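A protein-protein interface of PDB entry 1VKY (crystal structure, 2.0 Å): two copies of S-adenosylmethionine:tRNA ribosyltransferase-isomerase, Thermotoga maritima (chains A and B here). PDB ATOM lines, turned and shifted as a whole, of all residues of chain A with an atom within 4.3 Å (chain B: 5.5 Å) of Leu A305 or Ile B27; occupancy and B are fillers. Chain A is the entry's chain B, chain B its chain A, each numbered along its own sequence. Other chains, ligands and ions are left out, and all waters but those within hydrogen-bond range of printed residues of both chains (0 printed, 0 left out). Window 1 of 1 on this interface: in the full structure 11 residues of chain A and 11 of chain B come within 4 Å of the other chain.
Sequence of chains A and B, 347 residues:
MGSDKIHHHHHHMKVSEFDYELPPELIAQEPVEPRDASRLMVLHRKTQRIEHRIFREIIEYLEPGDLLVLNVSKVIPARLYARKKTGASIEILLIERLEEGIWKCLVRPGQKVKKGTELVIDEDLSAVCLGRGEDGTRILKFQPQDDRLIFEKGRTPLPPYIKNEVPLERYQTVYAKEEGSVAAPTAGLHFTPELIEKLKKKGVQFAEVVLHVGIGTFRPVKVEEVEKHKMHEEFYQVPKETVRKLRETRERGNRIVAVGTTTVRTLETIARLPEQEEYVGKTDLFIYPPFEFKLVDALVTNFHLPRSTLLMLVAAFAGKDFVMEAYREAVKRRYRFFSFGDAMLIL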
ATOM      1  N   TYR A  20     -17.086 -24.672 -38.434  1.00  0.00           N
ATOM      2  CA  TYR A  20     -18.052 -24.330 -39.459  1.00  0.00           C
ATOM      3  C   TYR A  20     -18.458 -22.915 -39.128  1.00  0.00           C
ATOM      4  O   TYR A  20     -18.195 -22.459 -38.034  1.00  0.00           O
ATOM      5  CB  TYR A  20     -19.255 -25.293 -39.460  1.00  0.00           C
ATOM      6  CG  TYR A  20     -20.143 -25.192 -38.240  1.00  0.00           C
ATOM      7  CD1 TYR A  20     -21.271 -24.368 -38.252  1.00  0.00           C
ATOM      8  CD2 TYR A  20     -19.869 -25.945 -37.063  1.00  0.00           C
ATOM      9  CE1 TYR A  20     -22.118 -24.280 -37.121  1.00  0.00           C
ATOM     10  CE2 TYR A  20     -20.723 -25.860 -35.923  1.00  0.00           C
ATOM     11  CZ  TYR A  20     -21.816 -24.997 -35.974  1.00  0.00           C
ATOM     12  OH  TYR A  20     -22.657 -24.863 -34.925  1.00  0.00           O
ATOM     13  N   LEU A  22     -20.811 -20.174 -38.084  1.00  0.00           N
ATOM     14  CA  LEU A  22     -22.081 -20.025 -37.365  1.00  0.00           C
ATOM     15  C   LEU A  22     -22.372 -18.519 -37.179  1.00  0.00           C
ATOM     16  O   LEU A  22     -21.704 -17.884 -36.345  1.00  0.00           O
ATOM     17  CB  LEU A  22     -21.975 -20.666 -35.982  1.00  0.00           C
ATOM     18  CG  LEU A  22     -23.175 -20.560 -35.035  1.00  0.00           C
ATOM     19  CD1 LEU A  22     -24.483 -20.903 -35.758  1.00  0.00           C
ATOM     20  CD2 LEU A  22     -23.004 -21.415 -33.744  1.00  0.00           C
ATOM     21  N   ILE A  27     -27.310 -18.149 -32.328  1.00  0.00           N
ATOM     22  CA  ILE A  27     -27.185 -18.686 -30.976  1.00  0.00           C
ATOM     23  C   ILE A  27     -28.306 -18.102 -30.119  1.00  0.00           C
ATOM     24  O   ILE A  27     -28.273 -16.942 -29.772  1.00  0.00           O
ATOM     25  CB  ILE A  27     -25.795 -18.416 -30.399  1.00  0.00           C
ATOM     26  CG1 ILE A  27     -24.731 -19.044 -31.305  1.00  0.00           C
ATOM     27  CG2 ILE A  27     -25.690 -18.902 -28.959  1.00  0.00           C
ATOM     28  CD1 ILE A  27     -23.345 -18.801 -30.877  1.00  0.00           C
ATOM     29  N   HIS A 304     -24.588 -27.996 -31.676  1.00  0.00           N
ATOM     30  CA  HIS A 304     -23.417 -27.650 -30.885  1.00  0.00           C
ATOM     31  C   HIS A 304     -22.553 -26.646 -31.619  1.00  0.00           C
ATOM     32  O   HIS A 304     -22.711 -26.448 -32.795  1.00  0.00           O
ATOM     33  CB  HIS A 304     -22.655 -28.913 -30.513  1.00  0.00           C
ATOM     34  CG  HIS A 304     -23.534 -29.965 -29.872  1.00  0.00           C
ATOM     35  ND1 HIS A 304     -24.104 -29.791 -28.631  1.00  0.00           N
ATOM     36  CD2 HIS A 304     -24.008 -31.147 -30.339  1.00  0.00           C
ATOM     37  CE1 HIS A 304     -24.863 -30.838 -28.342  1.00  0.00           C
ATOM     38  NE2 HIS A 304     -24.821 -31.675 -29.362  1.00  0.00           N
ATOM     39  N   LEU A 305     -21.623 -26.016 -30.907  1.00  0.00           N
ATOM     40  CA  LEU A 305     -20.852 -24.927 -31.465  1.00  0.00           C
ATOM     41  C   LEU A 305     -19.679 -25.451 -32.291  1.00  0.00           C
ATOM     42  O   LEU A 305     -19.181 -26.584 -32.035  1.00  0.00           O
ATOM     43  CB  LEU A 305     -20.364 -24.049 -30.290  1.00  0.00           C
ATOM     44  CG  LEU A 305     -21.442 -23.406 -29.378  1.00  0.00           C
ATOM     45  CD1 LEU A 305     -20.836 -22.825 -28.092  1.00  0.00           C
ATOM     46  CD2 LEU A 305     -22.182 -22.323 -30.165  1.00  0.00           C
ATOM     47  N   PRO A 306     -19.201 -24.631 -33.240  1.00  0.00           N
ATOM     48  CA  PRO A 306     -17.994 -24.933 -33.981  1.00  0.00           C
ATOM     49  C   PRO A 306     -16.877 -25.375 -33.079  1.00  0.00           C
ATOM     50  O   PRO A 306     -16.661 -24.813 -31.988  1.00  0.00           O
ATOM     51  CB  PRO A 306     -17.633 -23.593 -34.657  1.00  0.00           C
ATOM     52  CG  PRO A 306     -18.939 -22.870 -34.812  1.00  0.00           C
ATOM     53  CD  PRO A 306     -19.775 -23.327 -33.650  1.00  0.00           C
ATOM     54  N   ARG A 307     -16.217 -26.451 -33.502  1.00  0.00           N
ATOM     55  CA  ARG A 307     -15.042 -26.963 -32.809  1.00  0.00           C
ATOM     56  C   ARG A 307     -15.339 -27.540 -31.431  1.00  0.00           C
ATOM     57  O   ARG A 307     -14.402 -27.860 -30.713  1.00  0.00           O
ATOM     58  CB  ARG A 307     -13.956 -25.864 -32.677  1.00  0.00           C
ATOM     59  CG  ARG A 307     -13.501 -25.207 -34.020  1.00  0.00           C
ATOM     60  CD  ARG A 307     -12.608 -23.966 -33.827  1.00  0.00           C
ATOM     61  NE  ARG A 307     -13.429 -22.751 -33.944  1.00  0.00           N
ATOM     62  CZ  ARG A 307     -13.680 -21.855 -32.985  1.00  0.00           C
ATOM     63  NH1 ARG A 307     -13.143 -21.918 -31.766  1.00  0.00           N
ATOM     64  NH2 ARG A 307     -14.477 -20.851 -33.284  1.00  0.00           N
ATOM     65  N   SER A 308     -16.602 -27.697 -31.024  1.00  0.00           N
ATOM     66  CA  SER A 308     -16.838 -28.183 -29.660  1.00  0.00           C
ATOM     67  C   SER A 308     -16.574 -29.678 -29.590  1.00  0.00           C
ATOM     68  O   SER A 308     -16.791 -30.394 -30.590  1.00  0.00           O
ATOM     69  CB  SER A 308     -18.281 -27.979 -29.239  1.00  0.00           C
ATOM     70  OG  SER A 308     -19.115 -28.447 -30.261  1.00  0.00           O
ATOM     71  N   LEU A 311     -19.794 -31.484 -30.652  1.00  0.00           N
ATOM     72  CA  LEU A 311     -19.902 -31.669 -32.095  1.00  0.00           C
ATOM     73  C   LEU A 311     -19.076 -32.872 -32.538  1.00  0.00           C
ATOM     74  O   LEU A 311     -19.507 -33.687 -33.381  1.00  0.00           O
ATOM     75  CB  LEU A 311     -19.469 -30.373 -32.849  1.00  0.00           C
ATOM     76  CG  LEU A 311     -19.502 -30.464 -34.356  1.00  0.00           C
ATOM     77  CD1 LEU A 311     -20.858 -30.997 -34.852  1.00  0.00           C
ATOM     78  CD2 LEU A 311     -19.146 -29.092 -34.963  1.00  0.00           C
ATOM     79  N   PHE A 338     -27.280 -24.000 -29.924  1.00  0.00           N
ATOM     80  CA  PHE A 338     -26.855 -24.008 -28.541  1.00  0.00           C
ATOM     81  C   PHE A 338     -27.998 -24.355 -27.625  1.00  0.00           C
ATOM     82  O   PHE A 338     -29.000 -24.923 -28.052  1.00  0.00           O
ATOM     83  CB  PHE A 338     -26.092 -22.688 -28.213  1.00  0.00           C
ATOM     84  CG  PHE A 338     -25.152 -22.772 -27.064  1.00  0.00           C
ATOM     85  CD1 PHE A 338     -24.227 -23.790 -26.969  1.00  0.00           C
ATOM     86  CD2 PHE A 338     -25.209 -21.840 -26.044  1.00  0.00           C
ATOM     87  CE1 PHE A 338     -23.367 -23.852 -25.900  1.00  0.00           C
ATOM     88  CE2 PHE A 338     -24.338 -21.905 -24.975  1.00  0.00           C
ATOM     89  CZ  PHE A 338     -23.426 -22.892 -24.904  1.00  0.00           C
ATOM     90  N   LEU B  22     -12.802 -17.545 -30.194  1.00  0.00           N
ATOM     91  CA  LEU B  22     -13.497 -17.764 -28.951  1.00  0.00           C
ATOM     92  C   LEU B  22     -13.664 -19.263 -28.764  1.00  0.00           C
ATOM     93  O   LEU B  22     -14.450 -19.876 -29.491  1.00  0.00           O
ATOM     94  CB  LEU B  22     -14.873 -17.145 -29.011  1.00  0.00           C
ATOM     95  CG  LEU B  22     -15.767 -17.416 -27.787  1.00  0.00           C
ATOM     96  CD1 LEU B  22     -15.064 -17.073 -26.505  1.00  0.00           C
ATOM     97  CD2 LEU B  22     -17.093 -16.620 -27.931  1.00  0.00           C
ATOM     98  N   PRO B  23     -12.956 -19.868 -27.821  1.00  0.00           N
ATOM     99  CA  PRO B  23     -13.196 -21.302 -27.517  1.00  0.00           C
ATOM    100  C   PRO B  23     -14.610 -21.565 -27.084  1.00  0.00           C
ATOM    101  O   PRO B  23     -15.146 -20.834 -26.235  1.00  0.00           O
ATOM    102  CB  PRO B  23     -12.186 -21.617 -26.390  1.00  0.00           C
ATOM    103  CG  PRO B  23     -11.151 -20.566 -26.450  1.00  0.00           C
ATOM    104  CD  PRO B  23     -11.822 -19.320 -27.046  1.00  0.00           C
ATOM    105  N   PRO B  24     -15.254 -22.580 -27.681  1.00  0.00           N
ATOM    106  CA  PRO B  24     -16.646 -22.815 -27.412  1.00  0.00           C
ATOM    107  C   PRO B  24     -16.976 -23.059 -25.946  1.00  0.00           C
ATOM    108  O   PRO B  24     -18.040 -22.695 -25.507  1.00  0.00           O
ATOM    109  CB  PRO B  24     -17.007 -24.017 -28.320  1.00  0.00           C
ATOM    110  CG  PRO B  24     -15.713 -24.639 -28.691  1.00  0.00           C
ATOM    111  CD  PRO B  24     -14.726 -23.481 -28.732  1.00  0.00           C
ATOM    112  N   GLU B  25     -16.053 -23.604 -25.183  1.00  0.00           N
ATOM    113  CA  GLU B  25     -16.320 -23.879 -23.794  1.00  0.00           C
ATOM    114  C   GLU B  25     -16.419 -22.621 -22.957  1.00  0.00           C
ATOM    115  O   GLU B  25     -16.865 -22.675 -21.841  1.00  0.00           O
ATOM    116  CB  GLU B  25     -15.248 -24.808 -23.232  1.00  0.00           C
ATOM    117  CG  GLU B  25     -13.841 -24.250 -23.183  1.00  0.00           C
ATOM    118  CD  GLU B  25     -12.995 -24.478 -24.439  1.00  0.00           C
ATOM    119  OE1 GLU B  25     -13.524 -24.786 -25.540  1.00  0.00           O
ATOM    120  OE2 GLU B  25     -11.765 -24.277 -24.313  1.00  0.00           O
ATOM    121  N   LEU B  26     -15.997 -21.488 -23.495  1.00  0.00           N
ATOM    122  CA  LEU B  26     -16.118 -20.227 -22.735  1.00  0.00           C
ATOM    123  C   LEU B  26     -17.471 -19.562 -22.861  1.00  0.00           C
ATOM    124  O   LEU B  26     -17.750 -18.637 -22.100  1.00  0.00           O
ATOM    125  CB  LEU B  26     -15.030 -19.258 -23.104  1.00  0.00           C
ATOM    126  CG  LEU B  26     -13.613 -19.681 -22.767  1.00  0.00           C
ATOM    127  CD1 LEU B  26     -12.690 -18.508 -23.118  1.00  0.00           C
ATOM    128  CD2 LEU B  26     -13.402 -20.095 -21.339  1.00  0.00           C
ATOM    129  N   ILE B  27     -18.324 -20.040 -23.781  1.00  0.00           N
ATOM    130  CA  ILE B  27     -19.687 -19.550 -23.853  1.00  0.00           C
ATOM    131  C   ILE B  27     -20.548 -20.167 -22.760  1.00  0.00           C
ATOM    132  O   ILE B  27     -20.873 -21.386 -22.788  1.00  0.00           O
ATOM    133  CB  ILE B  27     -20.295 -19.765 -25.257  1.00  0.00           C
ATOM    134  CG1 ILE B  27     -19.400 -19.147 -26.292  1.00  0.00           C
ATOM    135  CG2 ILE B  27     -21.684 -19.202 -25.312  1.00  0.00           C
ATOM    136  CD1 ILE B  27     -19.846 -19.300 -27.743  1.00  0.00           C
ATOM    137  N   ALA B  28     -21.014 -19.329 -21.839  1.00  0.00           N
ATOM    138  CA  ALA B  28     -21.716 -19.850 -20.648  1.00  0.00           C
ATOM    139  C   ALA B  28     -23.151 -20.288 -20.952  1.00  0.00           C
ATOM    140  O   ALA B  28     -23.864 -19.648 -21.736  1.00  0.00           O
ATOM    141  CB  ALA B  28     -21.727 -18.837 -19.506  1.00  0.00           C
ATOM    142  N   GLN B  29     -23.571 -21.379 -20.311  1.00  0.00           N
ATOM    143  CA  GLN B  29     -24.924 -21.908 -20.450  1.00  0.00           C
ATOM    144  C   GLN B  29     -25.763 -21.441 -19.279  1.00  0.00           C
ATOM    145  O   GLN B  29     -26.979 -21.291 -19.391  1.00  0.00           O
ATOM    146  CB  GLN B  29     -24.897 -23.440 -20.460  1.00  0.00           C
ATOM    147  CG  GLN B  29     -23.971 -24.036 -21.507  1.00  0.00           C
ATOM    148  CD  GLN B  29     -24.058 -25.557 -21.583  1.00  0.00           C
ATOM    149  NE2 GLN B  29     -22.932 -26.217 -21.309  1.00  0.00           N
ATOM    150  N   LEU B 305     -20.155 -11.935 -29.087  1.00  0.00           N
ATOM    151  CA  LEU B 305     -19.601 -12.992 -29.950  1.00  0.00           C
ATOM    152  C   LEU B 305     -18.803 -12.430 -31.096  1.00  0.00           C
ATOM    153  O   LEU B 305     -19.076 -11.303 -31.560  1.00  0.00           O
ATOM    154  CB  LEU B 305     -20.732 -13.814 -30.545  1.00  0.00           C
ATOM    155  CG  LEU B 305     -21.605 -14.546 -29.522  1.00  0.00           C
ATOM    156  CD1 LEU B 305     -22.857 -15.152 -30.180  1.00  0.00           C
ATOM    157  CD2 LEU B 305     -20.798 -15.602 -28.782  1.00  0.00           C
ATOM    158  N   PHE B 337     -18.323 -15.875 -21.683  1.00  0.00           N
ATOM    159  CA  PHE B 337     -18.852 -15.030 -22.715  1.00  0.00           C
ATOM    160  C   PHE B 337     -20.367 -15.191 -22.912  1.00  0.00           C
ATOM    161  O   PHE B 337     -20.990 -16.162 -22.413  1.00  0.00           O
ATOM    162  CB  PHE B 337     -18.107 -15.291 -24.043  1.00  0.00           C
ATOM    163  CG  PHE B 337     -16.676 -14.740 -24.080  1.00  0.00           C
ATOM    164  CD1 PHE B 337     -15.653 -15.263 -23.263  1.00  0.00           C
ATOM    165  CD2 PHE B 337     -16.333 -13.740 -24.951  1.00  0.00           C
ATOM    166  CE1 PHE B 337     -14.390 -14.762 -23.288  1.00  0.00           C
ATOM    167  CE2 PHE B 337     -15.027 -13.267 -24.989  1.00  0.00           C
ATOM    168  CZ  PHE B 337     -14.066 -13.766 -24.171  1.00  0.00           C
ATOM    169  N   PHE B 338     -20.954 -14.219 -23.637  1.00  0.00           N
ATOM    170  CA  PHE B 338     -22.342 -14.224 -24.055  1.00  0.00           C
ATOM    171  C   PHE B 338     -23.288 -13.933 -22.875  1.00  0.00           C
ATOM    172  O   PHE B 338     -22.837 -13.481 -21.831  1.00  0.00           O
ATOM    173  CB  PHE B 338     -22.640 -15.505 -24.835  1.00  0.00           C
ATOM    174  CG  PHE B 338     -23.870 -15.476 -25.721  1.00  0.00           C
ATOM    175  CD1 PHE B 338     -24.055 -14.507 -26.673  1.00  0.00           C
ATOM    176  CD2 PHE B 338     -24.833 -16.468 -25.594  1.00  0.00           C
ATOM    177  CE1 PHE B 338     -25.168 -14.514 -27.480  1.00  0.00           C
ATOM    178  CE2 PHE B 338     -25.975 -16.454 -26.405  1.00  0.00           C
ATOM    179  CZ  PHE B 338     -26.123 -15.501 -27.342  1.00  0.00           C
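CD1 of Ile A27 touches CD1 of Leu B305, 3.7 Å away. CG2 of Ile A27 touches CE2 of Phe B338, at 3.5 Å. Leu A305 touches Pro B24 (CD1 to O, 3.8 Å). CD1 of Ile B27 touches CD1 of Leu A305, 3.7 Å away. Pro A306 touches Pro B24. NH1 of Arg A307 touches CD of Pro B24, at 3.8 Å. CA of Ser A308 touches CG of Pro B24 (3.8 Å). CZ of Phe A338 touches O of Ile B27, 3.6 Å away. Ala B28 touches Phe A338 (O to CE2, 3.98 Å). Phe A338 touches Gln B29.
Hydrophobic or aromatic side chains of chain B that line the printed part of chain A: Pro B24, Ile B27, Leu B305 and Phe B338. Among the printed residues, no Asp or Glu carboxylate lies within 4 Å of a Lys or Arg side-chain nitrogen of the other chain.
Leu A305 touches just these residues of chain B: Pro B24 (3.8 Å) and Ile B27 (3.7 Å). Of the printed residues of chain B, Pro A306 touches Pro B24. Of the printed residues of chain B, Arg A307 touches Leu B22 (3.3 Å) and Pro B24 (3.8 Å). Printed residues of chain B within 4 Å of Phe A338: Ile B27, Ala B28 and Gln B29. Of chain A, only Leu A305 (3.7 Å) and Phe A338 (3.6 Å) come within 4 Å of Ile B27. Of the printed residues of chain A, Ala B28 touches Phe A338. Of the printed residues of chain A, Leu B305 touches Ile A27 (3.7 Å). The nearest printed residue of chain B that does not touch Leu A305 is Glu B25 (5.7 Å). The nearest printed residue of chain A that does not touch Ile B27 is Ile A27 (4.7 Å). The nearest printed residue of chain A that does not touch Leu B22 is Pro A306 (6.0 Å).
Ile A27 touches Leu B305, and with the chains exchanged Leu A305 touches Ile B27. Ile A27 touches Phe B338, and with the chains exchanged Phe A338 touches Ile B27.
The backbone NH (N) of Ala B28 is in hydrogen-bond range of the backbone carbonyl oxygen (O) of Phe B337 (3.2 Å). OG of Ser A308 lies within hydrogen-bond range of O of Leu A305, at 2.6 Å. The backbone NH of Leu A311 sits at hydrogen-bond distance from the side-chain hydroxyl of Ser A308, at 3.1 Å.
O of Leu B22 is in hydrogen-bond range of NH1 of Arg A307.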
